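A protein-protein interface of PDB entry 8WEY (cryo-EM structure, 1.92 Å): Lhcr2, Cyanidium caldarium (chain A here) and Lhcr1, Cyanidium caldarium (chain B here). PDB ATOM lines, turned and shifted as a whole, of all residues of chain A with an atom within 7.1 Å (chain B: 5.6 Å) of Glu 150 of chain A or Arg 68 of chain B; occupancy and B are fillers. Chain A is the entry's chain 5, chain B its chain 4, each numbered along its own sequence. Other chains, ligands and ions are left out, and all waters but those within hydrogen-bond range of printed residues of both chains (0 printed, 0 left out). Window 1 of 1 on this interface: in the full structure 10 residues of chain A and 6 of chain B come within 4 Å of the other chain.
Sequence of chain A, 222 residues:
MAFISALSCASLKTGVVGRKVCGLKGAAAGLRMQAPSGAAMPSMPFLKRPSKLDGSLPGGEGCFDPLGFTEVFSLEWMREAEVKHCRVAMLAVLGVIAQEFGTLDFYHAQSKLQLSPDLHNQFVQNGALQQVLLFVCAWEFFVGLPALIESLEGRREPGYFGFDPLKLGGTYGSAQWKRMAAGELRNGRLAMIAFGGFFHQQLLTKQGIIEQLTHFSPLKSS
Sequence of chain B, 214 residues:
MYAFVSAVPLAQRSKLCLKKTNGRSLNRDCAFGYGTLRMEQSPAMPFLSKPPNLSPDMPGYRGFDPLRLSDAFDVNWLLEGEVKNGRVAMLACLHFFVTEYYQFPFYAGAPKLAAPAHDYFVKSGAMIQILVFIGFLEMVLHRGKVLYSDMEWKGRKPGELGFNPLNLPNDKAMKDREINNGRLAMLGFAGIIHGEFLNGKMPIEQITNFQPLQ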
ATOM      1  N   GLY A 144      23.585 -20.317  18.292  1.00  0.00           N
ATOM      2  CA  GLY A 144      24.062 -21.714  18.262  1.00  0.00           C
ATOM      3  C   GLY A 144      23.002 -22.706  18.722  1.00  0.00           C
ATOM      4  O   GLY A 144      22.872 -23.766  18.077  1.00  0.00           O
ATOM      5  N   LEU A 145      22.282 -22.390  19.803  1.00  0.00           N
ATOM      6  CA  LEU A 145      21.267 -23.295  20.404  1.00  0.00           C
ATOM      7  C   LEU A 145      20.001 -23.305  19.546  1.00  0.00           C
ATOM      8  O   LEU A 145      19.485 -24.382  19.261  1.00  0.00           O
ATOM      9  CB  LEU A 145      21.000 -22.896  21.863  1.00  0.00           C
ATOM     10  CG  LEU A 145      19.947 -23.721  22.601  1.00  0.00           C
ATOM     11  CD1 LEU A 145      20.260 -25.211  22.522  1.00  0.00           C
ATOM     12  CD2 LEU A 145      19.849 -23.287  24.053  1.00  0.00           C
ATOM     13  N   PRO A 146      19.436 -22.145  19.122  1.00  0.00           N
ATOM     14  CA  PRO A 146      18.373 -22.135  18.113  1.00  0.00           C
ATOM     15  C   PRO A 146      18.742 -22.880  16.825  1.00  0.00           C
ATOM     16  O   PRO A 146      17.907 -23.609  16.321  1.00  0.00           O
ATOM     17  CB  PRO A 146      18.172 -20.643  17.807  1.00  0.00           C
ATOM     18  CG  PRO A 146      18.564 -19.956  19.093  1.00  0.00           C
ATOM     19  CD  PRO A 146      19.693 -20.796  19.654  1.00  0.00           C
ATOM     20  N   ALA A 147      19.969 -22.674  16.339  1.00  0.00           N
ATOM     21  CA  ALA A 147      20.537 -23.307  15.124  1.00  0.00           C
ATOM     22  C   ALA A 147      20.587 -24.829  15.299  1.00  0.00           C
ATOM     23  O   ALA A 147      20.214 -25.540  14.351  1.00  0.00           O
ATOM     24  CB  ALA A 147      21.904 -22.732  14.830  1.00  0.00           C
ATOM     25  N   LEU A 148      21.039 -25.309  16.462  1.00  0.00           N
ATOM     26  CA  LEU A 148      21.125 -26.761  16.785  1.00  0.00           C
ATOM     27  C   LEU A 148      19.714 -27.368  16.790  1.00  0.00           C
ATOM     28  O   LEU A 148      19.528 -28.413  16.148  1.00  0.00           O
ATOM     29  CB  LEU A 148      21.826 -26.948  18.137  1.00  0.00           C
ATOM     30  CG  LEU A 148      21.880 -28.374  18.685  1.00  0.00           C
ATOM     31  CD1 LEU A 148      22.411 -29.363  17.652  1.00  0.00           C
ATOM     32  CD2 LEU A 148      22.729 -28.414  19.945  1.00  0.00           C
ATOM     33  N   ILE A 149      18.758 -26.723  17.462  1.00  0.00           N
ATOM     34  CA  ILE A 149      17.345 -27.199  17.598  1.00  0.00           C
ATOM     35  C   ILE A 149      16.702 -27.298  16.205  1.00  0.00           C
ATOM     36  O   ILE A 149      16.004 -28.300  15.959  1.00  0.00           O
ATOM     37  CB  ILE A 149      16.544 -26.295  18.560  1.00  0.00           C
ATOM     38  CG1 ILE A 149      17.048 -26.433  20.001  1.00  0.00           C
ATOM     39  CG2 ILE A 149      15.051 -26.574  18.466  1.00  0.00           C
ATOM     40  CD1 ILE A 149      16.663 -25.282  20.903  1.00  0.00           C
ATOM     41  N   GLU A 150      16.926 -26.307  15.334  1.00  0.00           N
ATOM     42  CA  GLU A 150      16.462 -26.308  13.916  1.00  0.00           C
ATOM     43  C   GLU A 150      16.976 -27.562  13.196  1.00  0.00           C
ATOM     44  O   GLU A 150      16.179 -28.180  12.464  1.00  0.00           O
ATOM     45  CB  GLU A 150      16.929 -25.053  13.171  1.00  0.00           C
ATOM     46  CG  GLU A 150      16.134 -23.807  13.521  1.00  0.00           C
ATOM     47  CD  GLU A 150      14.740 -23.699  12.917  1.00  0.00           C
ATOM     48  OE1 GLU A 150      14.330 -24.620  12.179  1.00  0.00           O
ATOM     49  OE2 GLU A 150      14.059 -22.692  13.200  1.00  0.00           O
ATOM     50  N   SER A 151      18.249 -27.920  13.397  1.00  0.00           N
ATOM     51  CA  SER A 151      18.922 -29.079  12.751  1.00  0.00           C
ATOM     52  C   SER A 151      18.336 -30.398  13.262  1.00  0.00           C
ATOM     53  O   SER A 151      18.202 -31.326  12.440  1.00  0.00           O
ATOM     54  CB  SER A 151      20.416 -29.038  12.947  1.00  0.00           C
ATOM     55  OG  SER A 151      20.975 -27.895  12.327  1.00  0.00           O
ATOM     56  N   LEU A 152      17.998 -30.481  14.554  1.00  0.00           N
ATOM     57  CA  LEU A 152      17.415 -31.700  15.181  1.00  0.00           C
ATOM     58  C   LEU A 152      15.991 -31.920  14.654  1.00  0.00           C
ATOM     59  O   LEU A 152      15.622 -33.092  14.434  1.00  0.00           O
ATOM     60  CB  LEU A 152      17.437 -31.560  16.708  1.00  0.00           C
ATOM     61  CG  LEU A 152      18.820 -31.415  17.346  1.00  0.00           C
ATOM     62  CD1 LEU A 152      18.723 -31.393  18.864  1.00  0.00           C
ATOM     63  CD2 LEU A 152      19.766 -32.509  16.878  1.00  0.00           C
ATOM     64  N   GLU A 153      15.235 -30.837  14.447  1.00  0.00           N
ATOM     65  CA  GLU A 153      13.887 -30.850  13.807  1.00  0.00           C
ATOM     66  C   GLU A 153      14.003 -31.242  12.326  1.00  0.00           C
ATOM     67  O   GLU A 153      13.004 -31.749  11.780  1.00  0.00           O
ATOM     68  CB  GLU A 153      13.196 -29.493  13.967  1.00  0.00           C
ATOM     69  CG  GLU A 153      12.323 -29.397  15.212  1.00  0.00           C
ATOM     70  CD  GLU A 153      12.452 -28.107  16.008  1.00  0.00           C
ATOM     71  OE1 GLU A 153      12.448 -27.019  15.392  1.00  0.00           O
ATOM     72  OE2 GLU A 153      12.546 -28.197  17.249  1.00  0.00           O
ATOM     73  N   GLY A 154      15.164 -31.004  11.704  1.00  0.00           N
ATOM     74  CA  GLY A 154      15.479 -31.384  10.311  1.00  0.00           C
ATOM     75  C   GLY A 154      15.166 -30.266   9.327  1.00  0.00           C
ATOM     76  O   GLY A 154      14.807 -30.585   8.176  1.00  0.00           O
ATOM     77  N   ARG A 155      15.314 -29.011   9.762  1.00  0.00           N
ATOM     78  CA  ARG A 155      14.999 -27.777   8.992  1.00  0.00           C
ATOM     79  C   ARG A 155      16.274 -26.948   8.757  1.00  0.00           C
ATOM     80  O   ARG A 155      16.150 -25.799   8.284  1.00  0.00           O
ATOM     81  CB  ARG A 155      13.941 -26.977   9.759  1.00  0.00           C
ATOM     82  CG  ARG A 155      12.557 -27.604   9.751  1.00  0.00           C
ATOM     83  CD  ARG A 155      11.494 -26.546   9.975  1.00  0.00           C
ATOM     84  NE  ARG A 155      11.679 -25.825  11.232  1.00  0.00           N
ATOM     85  CZ  ARG A 155      11.221 -26.211  12.429  1.00  0.00           C
ATOM     86  NH1 ARG A 155      10.561 -27.351  12.583  1.00  0.00           N
ATOM     87  NH2 ARG A 155      11.436 -25.445  13.486  1.00  0.00           N
ATOM     88  N   ARG A 156      17.451 -27.514   9.051  1.00  0.00           N
ATOM     89  CA  ARG A 156      18.776 -26.861   8.879  1.00  0.00           C
ATOM     90  C   ARG A 156      19.848 -27.947   8.727  1.00  0.00           C
ATOM     91  O   ARG A 156      19.826 -28.903   9.519  1.00  0.00           O
ATOM     92  CB  ARG A 156      19.075 -25.935  10.066  1.00  0.00           C
ATOM     93  CG  ARG A 156      20.498 -25.387  10.095  1.00  0.00           C
ATOM     94  CD  ARG A 156      20.686 -24.301  11.132  1.00  0.00           C
ATOM     95  NE  ARG A 156      22.091 -23.997  11.371  1.00  0.00           N
ATOM     96  CZ  ARG A 156      22.946 -24.738  12.083  1.00  0.00           C
ATOM     97  NH1 ARG A 156      22.559 -25.863  12.663  1.00  0.00           N
ATOM     98  NH2 ARG A 156      24.200 -24.337  12.218  1.00  0.00           N
ATOM     99  N   GLU A 157      20.743 -27.806   7.746  1.00  0.00           N
ATOM    100  CA  GLU A 157      21.941 -28.675   7.602  1.00  0.00           C
ATOM    101  C   GLU A 157      22.927 -28.289   8.701  1.00  0.00           C
ATOM    102  O   GLU A 157      23.229 -27.108   8.854  1.00  0.00           O
ATOM    103  CB  GLU A 157      22.571 -28.534   6.216  1.00  0.00           C
ATOM    104  CG  GLU A 157      23.605 -29.607   5.918  1.00  0.00           C
ATOM    105  CD  GLU A 157      24.316 -29.471   4.582  1.00  0.00           C
ATOM    106  OE1 GLU A 157      24.713 -28.340   4.233  1.00  0.00           O
ATOM    107  OE2 GLU A 157      24.479 -30.501   3.895  1.00  0.00           O
ATOM    108  N   PHE B  47      19.418 -18.974   7.975  1.00  0.00           N
ATOM    109  CA  PHE B  47      19.711 -20.335   8.508  1.00  0.00           C
ATOM    110  C   PHE B  47      18.591 -20.823   9.442  1.00  0.00           C
ATOM    111  O   PHE B  47      18.377 -22.051   9.488  1.00  0.00           O
ATOM    112  CB  PHE B  47      21.075 -20.365   9.203  1.00  0.00           C
ATOM    113  CG  PHE B  47      21.277 -19.352  10.303  1.00  0.00           C
ATOM    114  CD1 PHE B  47      21.740 -18.075  10.017  1.00  0.00           C
ATOM    115  CD2 PHE B  47      21.044 -19.684  11.629  1.00  0.00           C
ATOM    116  CE1 PHE B  47      21.939 -17.146  11.026  1.00  0.00           C
ATOM    117  CE2 PHE B  47      21.247 -18.755  12.639  1.00  0.00           C
ATOM    118  CZ  PHE B  47      21.691 -17.488  12.334  1.00  0.00           C
ATOM    119  N   LEU B  48      17.912 -19.918  10.158  1.00  0.00           N
ATOM    120  CA  LEU B  48      16.715 -20.238  10.988  1.00  0.00           C
ATOM    121  C   LEU B  48      15.447 -20.096  10.138  1.00  0.00           C
ATOM    122  O   LEU B  48      15.403 -19.194   9.277  1.00  0.00           O
ATOM    123  CB  LEU B  48      16.640 -19.306  12.202  1.00  0.00           C
ATOM    124  CG  LEU B  48      17.863 -19.274  13.118  1.00  0.00           C
ATOM    125  CD1 LEU B  48      17.582 -18.437  14.354  1.00  0.00           C
ATOM    126  CD2 LEU B  48      18.308 -20.673  13.524  1.00  0.00           C
ATOM    127  N   SER B  49      14.457 -20.961  10.387  1.00  0.00           N
ATOM    128  CA  SER B  49      13.079 -20.885   9.832  1.00  0.00           C
ATOM    129  C   SER B  49      12.401 -19.599  10.321  1.00  0.00           C
ATOM    130  O   SER B  49      12.778 -19.101  11.404  1.00  0.00           O
ATOM    131  CB  SER B  49      12.266 -22.101  10.207  1.00  0.00           C
ATOM    132  OG  SER B  49      12.878 -23.294   9.738  1.00  0.00           O
ATOM    133  N   LYS B  50      11.426 -19.098   9.558  1.00  0.00           N
ATOM    134  CA  LYS B  50      10.681 -17.842   9.850  1.00  0.00           C
ATOM    135  C   LYS B  50       9.851 -18.049  11.115  1.00  0.00           C
ATOM    136  O   LYS B  50       9.176 -19.071  11.234  1.00  0.00           O
ATOM    137  CB  LYS B  50       9.783 -17.461   8.668  1.00  0.00           C
ATOM    138  CG  LYS B  50       9.260 -16.030   8.674  1.00  0.00           C
ATOM    139  CD  LYS B  50       7.982 -15.854   7.876  1.00  0.00           C
ATOM    140  CE  LYS B  50       6.729 -16.161   8.671  1.00  0.00           C
ATOM    141  NZ  LYS B  50       6.423 -15.101   9.662  1.00  0.00           N
ATOM    142  N   PRO B  51       9.894 -17.123  12.105  1.00  0.00           N
ATOM    143  CA  PRO B  51       8.945 -17.140  13.221  1.00  0.00           C
ATOM    144  C   PRO B  51       7.507 -17.086  12.702  1.00  0.00           C
ATOM    145  O   PRO B  51       7.111 -16.079  12.118  1.00  0.00           O
ATOM    146  CB  PRO B  51       9.301 -15.885  14.036  1.00  0.00           C
ATOM    147  CG  PRO B  51      10.743 -15.602  13.681  1.00  0.00           C
ATOM    148  CD  PRO B  51      10.886 -16.043  12.239  1.00  0.00           C
ATOM    149  N   PRO B  52       6.695 -18.163  12.858  1.00  0.00           N
ATOM    150  CA  PRO B  52       5.380 -18.239  12.210  1.00  0.00           C
ATOM    151  C   PRO B  52       4.398 -17.111  12.569  1.00  0.00           C
ATOM    152  O   PRO B  52       3.734 -16.617  11.676  1.00  0.00           O
ATOM    153  CB  PRO B  52       4.803 -19.579  12.699  1.00  0.00           C
ATOM    154  CG  PRO B  52       6.015 -20.390  13.102  1.00  0.00           C
ATOM    155  CD  PRO B  52       6.995 -19.373  13.644  1.00  0.00           C
ATOM    156  N   ASP B  65      13.422 -13.512  15.672  1.00  0.00           N
ATOM    157  CA  ASP B  65      12.985 -14.127  16.955  1.00  0.00           C
ATOM    158  C   ASP B  65      13.656 -15.493  17.098  1.00  0.00           C
ATOM    159  O   ASP B  65      12.991 -16.525  17.003  1.00  0.00           O
ATOM    160  CB  ASP B  65      11.457 -14.227  17.030  1.00  0.00           C
ATOM    161  CG  ASP B  65      10.908 -14.549  18.416  1.00  0.00           C
ATOM    162  OD1 ASP B  65      11.711 -14.802  19.337  1.00  0.00           O
ATOM    163  OD2 ASP B  65       9.675 -14.540  18.570  1.00  0.00           O
ATOM    164  N   PRO B  66      14.994 -15.552  17.303  1.00  0.00           N
ATOM    165  CA  PRO B  66      15.682 -16.831  17.483  1.00  0.00           C
ATOM    166  C   PRO B  66      15.216 -17.649  18.700  1.00  0.00           C
ATOM    167  O   PRO B  66      15.217 -18.864  18.599  1.00  0.00           O
ATOM    168  CB  PRO B  66      17.165 -16.446  17.613  1.00  0.00           C
ATOM    169  CG  PRO B  66      17.151 -14.984  17.997  1.00  0.00           C
ATOM    170  CD  PRO B  66      15.928 -14.414  17.314  1.00  0.00           C
ATOM    171  N   LEU B  67      14.821 -16.990  19.797  1.00  0.00           N
ATOM    172  CA  LEU B  67      14.316 -17.656  21.035  1.00  0.00           C
ATOM    173  C   LEU B  67      12.850 -18.090  20.867  1.00  0.00           C
ATOM    174  O   LEU B  67      12.393 -18.888  21.709  1.00  0.00           O
ATOM    175  CB  LEU B  67      14.457 -16.720  22.241  1.00  0.00           C
ATOM    176  CG  LEU B  67      15.882 -16.420  22.710  1.00  0.00           C
ATOM    177  CD1 LEU B  67      15.857 -15.655  24.025  1.00  0.00           C
ATOM    178  CD2 LEU B  67      16.707 -17.696  22.843  1.00  0.00           C
ATOM    179  N   ARG B  68      12.142 -17.582  19.850  1.00  0.00           N
ATOM    180  CA  ARG B  68      10.722 -17.902  19.535  1.00  0.00           C
ATOM    181  C   ARG B  68       9.839 -17.539  20.739  1.00  0.00           C
ATOM    182  O   ARG B  68       9.027 -18.385  21.174  1.00  0.00           O
ATOM    183  CB  ARG B  68      10.579 -19.371  19.115  1.00  0.00           C
ATOM    184  CG  ARG B  68      11.246 -19.708  17.788  1.00  0.00           C
ATOM    185  CD  ARG B  68      10.581 -19.014  16.611  1.00  0.00           C
ATOM    186  NE  ARG B  68      10.900 -19.643  15.334  1.00  0.00           N
ATOM    187  CZ  ARG B  68      10.346 -20.763  14.858  1.00  0.00           C
ATOM    188  NH1 ARG B  68       9.428 -21.421  15.546  1.00  0.00           N
ATOM    189  NH2 ARG B  68      10.723 -21.234  13.683  1.00  0.00           N
ATOM    190  N   LEU B  69      10.000 -16.316  21.253  1.00  0.00           N
ATOM    191  CA  LEU B  69       9.152 -15.739  22.331  1.00  0.00           C
ATOM    192  C   LEU B  69       7.754 -15.434  21.773  1.00  0.00           C
ATOM    193  O   LEU B  69       6.792 -15.428  22.573  1.00  0.00           O
ATOM    194  CB  LEU B  69       9.827 -14.480  22.888  1.00  0.00           C
ATOM    195  CG  LEU B  69      11.166 -14.707  23.592  1.00  0.00           C
ATOM    196  CD1 LEU B  69      11.907 -13.395  23.795  1.00  0.00           C
ATOM    197  CD2 LEU B  69      10.969 -15.416  24.925  1.00  0.00           C
ATOM    198  N   SER B  70       7.641 -15.211  20.455  1.00  0.00           N
ATOM    199  CA  SER B  70       6.365 -15.009  19.715  1.00  0.00           C
ATOM    200  C   SER B  70       5.521 -16.291  19.702  1.00  0.00           C
ATOM    201  O   SER B  70       4.307 -16.175  19.437  1.00  0.00           O
ATOM    202  CB  SER B  70       6.623 -14.512  18.317  1.00  0.00           C
ATOM    203  OG  SER B  70       7.404 -15.436  17.573  1.00  0.00           O
ATOM    204  N   ASP B  71       6.128 -17.460  19.938  1.00  0.00           N
ATOM    205  CA  ASP B  71       5.419 -18.751  20.162  1.00  0.00           C
ATOM    206  C   ASP B  71       4.955 -18.834  21.623  1.00  0.00           C
ATOM    207  O   ASP B  71       3.836 -19.337  21.853  1.00  0.00           O
ATOM    208  CB  ASP B  71       6.307 -19.952  19.820  1.00  0.00           C
ATOM    209  CG  ASP B  71       6.797 -19.990  18.382  1.00  0.00           C
ATOM    210  OD1 ASP B  71       6.450 -19.069  17.613  1.00  0.00           O
ATOM    211  OD2 ASP B  71       7.523 -20.945  18.041  1.00  0.00           O
ATOM    212  N   ALA B  72       5.787 -18.374  22.563  1.00  0.00           N
ATOM    213  CA  ALA B  72       5.555 -18.433  24.028  1.00  0.00           C
ATOM    214  C   ALA B  72       4.468 -17.434  24.445  1.00  0.00           C
ATOM    215  O   ALA B  72       3.660 -17.788  25.328  1.00  0.00           O
ATOM    216  CB  ALA B  72       6.845 -18.166  24.768  1.00  0.00           C
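OG of Ser 49 of chain B is in hydrogen-bond range of OE1 of Glu 150 of chain A, at 3.1 Å.
OG of Ser 49 of chain B is in hydrogen-bond range of NE of Arg 155 of chain A, 3.2 Å away.
OE2 of Glu 150 of chain A lies within salt-bridge range of NH2 of Arg 68 of chain B (3.7 Å).
Of the 14 printed residues of chain A, 5 touch a printed residue of chain B.
Printed residues of chain A that touch a printed residue of chain B: Pro 146, Ala 147, Glu 150, Arg 155 and Arg 156.
Hydrophobic or aromatic side chains of chain A within 4 Å of the printed part of chain B: Pro 146.
Hydrophobic or aromatic side chains of chain B within 4 Å of the printed part of chain A: Leu 48.
Among the printed residues, 8 pairs touch across the chains.
Among the printed residues, Asp or Glu carboxylates within 4 Å of a Lys or Arg side-chain nitrogen of the other chain: Glu 150 of chain A with Arg 68 of chain B.
Among the printed residues, merely in contact across the chains: Pro 146 of chain A with Pro 66 of chain B, Arg 156 of chain A with Phe 47 of chain B, Ala 147 of chain A with Leu 48 of chain B, Glu 150 of chain A with Leu 48 of chain B and Pro 146 of chain A with Leu 48 of chain B.
Glu 150 of chain A touches just these residues of chain B: Leu 48 (3.8 Å), Ser 49 (3.1 Å) and Arg 68 (3.7 Å).
Arg 68 of chain B touches just one residue of chain A: Glu 150 (3.7 Å).
Of the printed residues of chain A, Leu 48 of chain B touches Pro 146, Ala 147 and Glu 150.
Of the printed residues of chain A, Phe 47 of chain B touches Arg 156 (3.6 Å).
Of the printed residues of chain B, Arg 155 of chain A touches Ser 49.
Of the printed residues of chain A, Pro 66 of chain B touches Pro 146 (3.5 Å).
Of the printed residues of chain B, Pro 146 of chain A touches Leu 48 and Pro 66.
Ser 70 of chain B touches none of the printed residues of chain A.
The nearest residue of chain B that does not touch Glu 150 of chain A is Phe 47 of chain B (4.9 Å).
The nearest residue of chain A that does not touch Arg 68 of chain B is Arg 155 of chain A (4.3 Å).
The nearest printed residue of chain B that does not touch Arg 156 of chain A is Leu 48 of chain B (5.0 Å).
The backbone NH of Arg 68 of chain B is in hydrogen-bond range of the side-chain carboxylate of Asp 65 of chain B (2.9 Å).
The side-chain carboxylate (OD2) of Asp 71 of chain B is in salt-bridge range of the guanidinium group (NH1) of Arg 68 of chain B (3.2 Å).
The backbone carbonyl oxygen (O) of Ala 147 of chain A sits at hydrogen-bond distance from the side-chain hydroxyl (OG) of Ser 151 of chain A (3.2 Å).
OE1 of Glu 150 of chain A is in salt-bridge range of NE of Arg 155 of chain A, at 3.1 Å.
NH1 of Arg 156 of chain A sits at hydrogen-bond distance from OG of Ser 151 of chain A.
The side-chain carboxylate (OE1) of Glu 153 of chain A is in salt-bridge range of the guanidinium group (NH2) of Arg 155 of chain A (2.7 Å).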
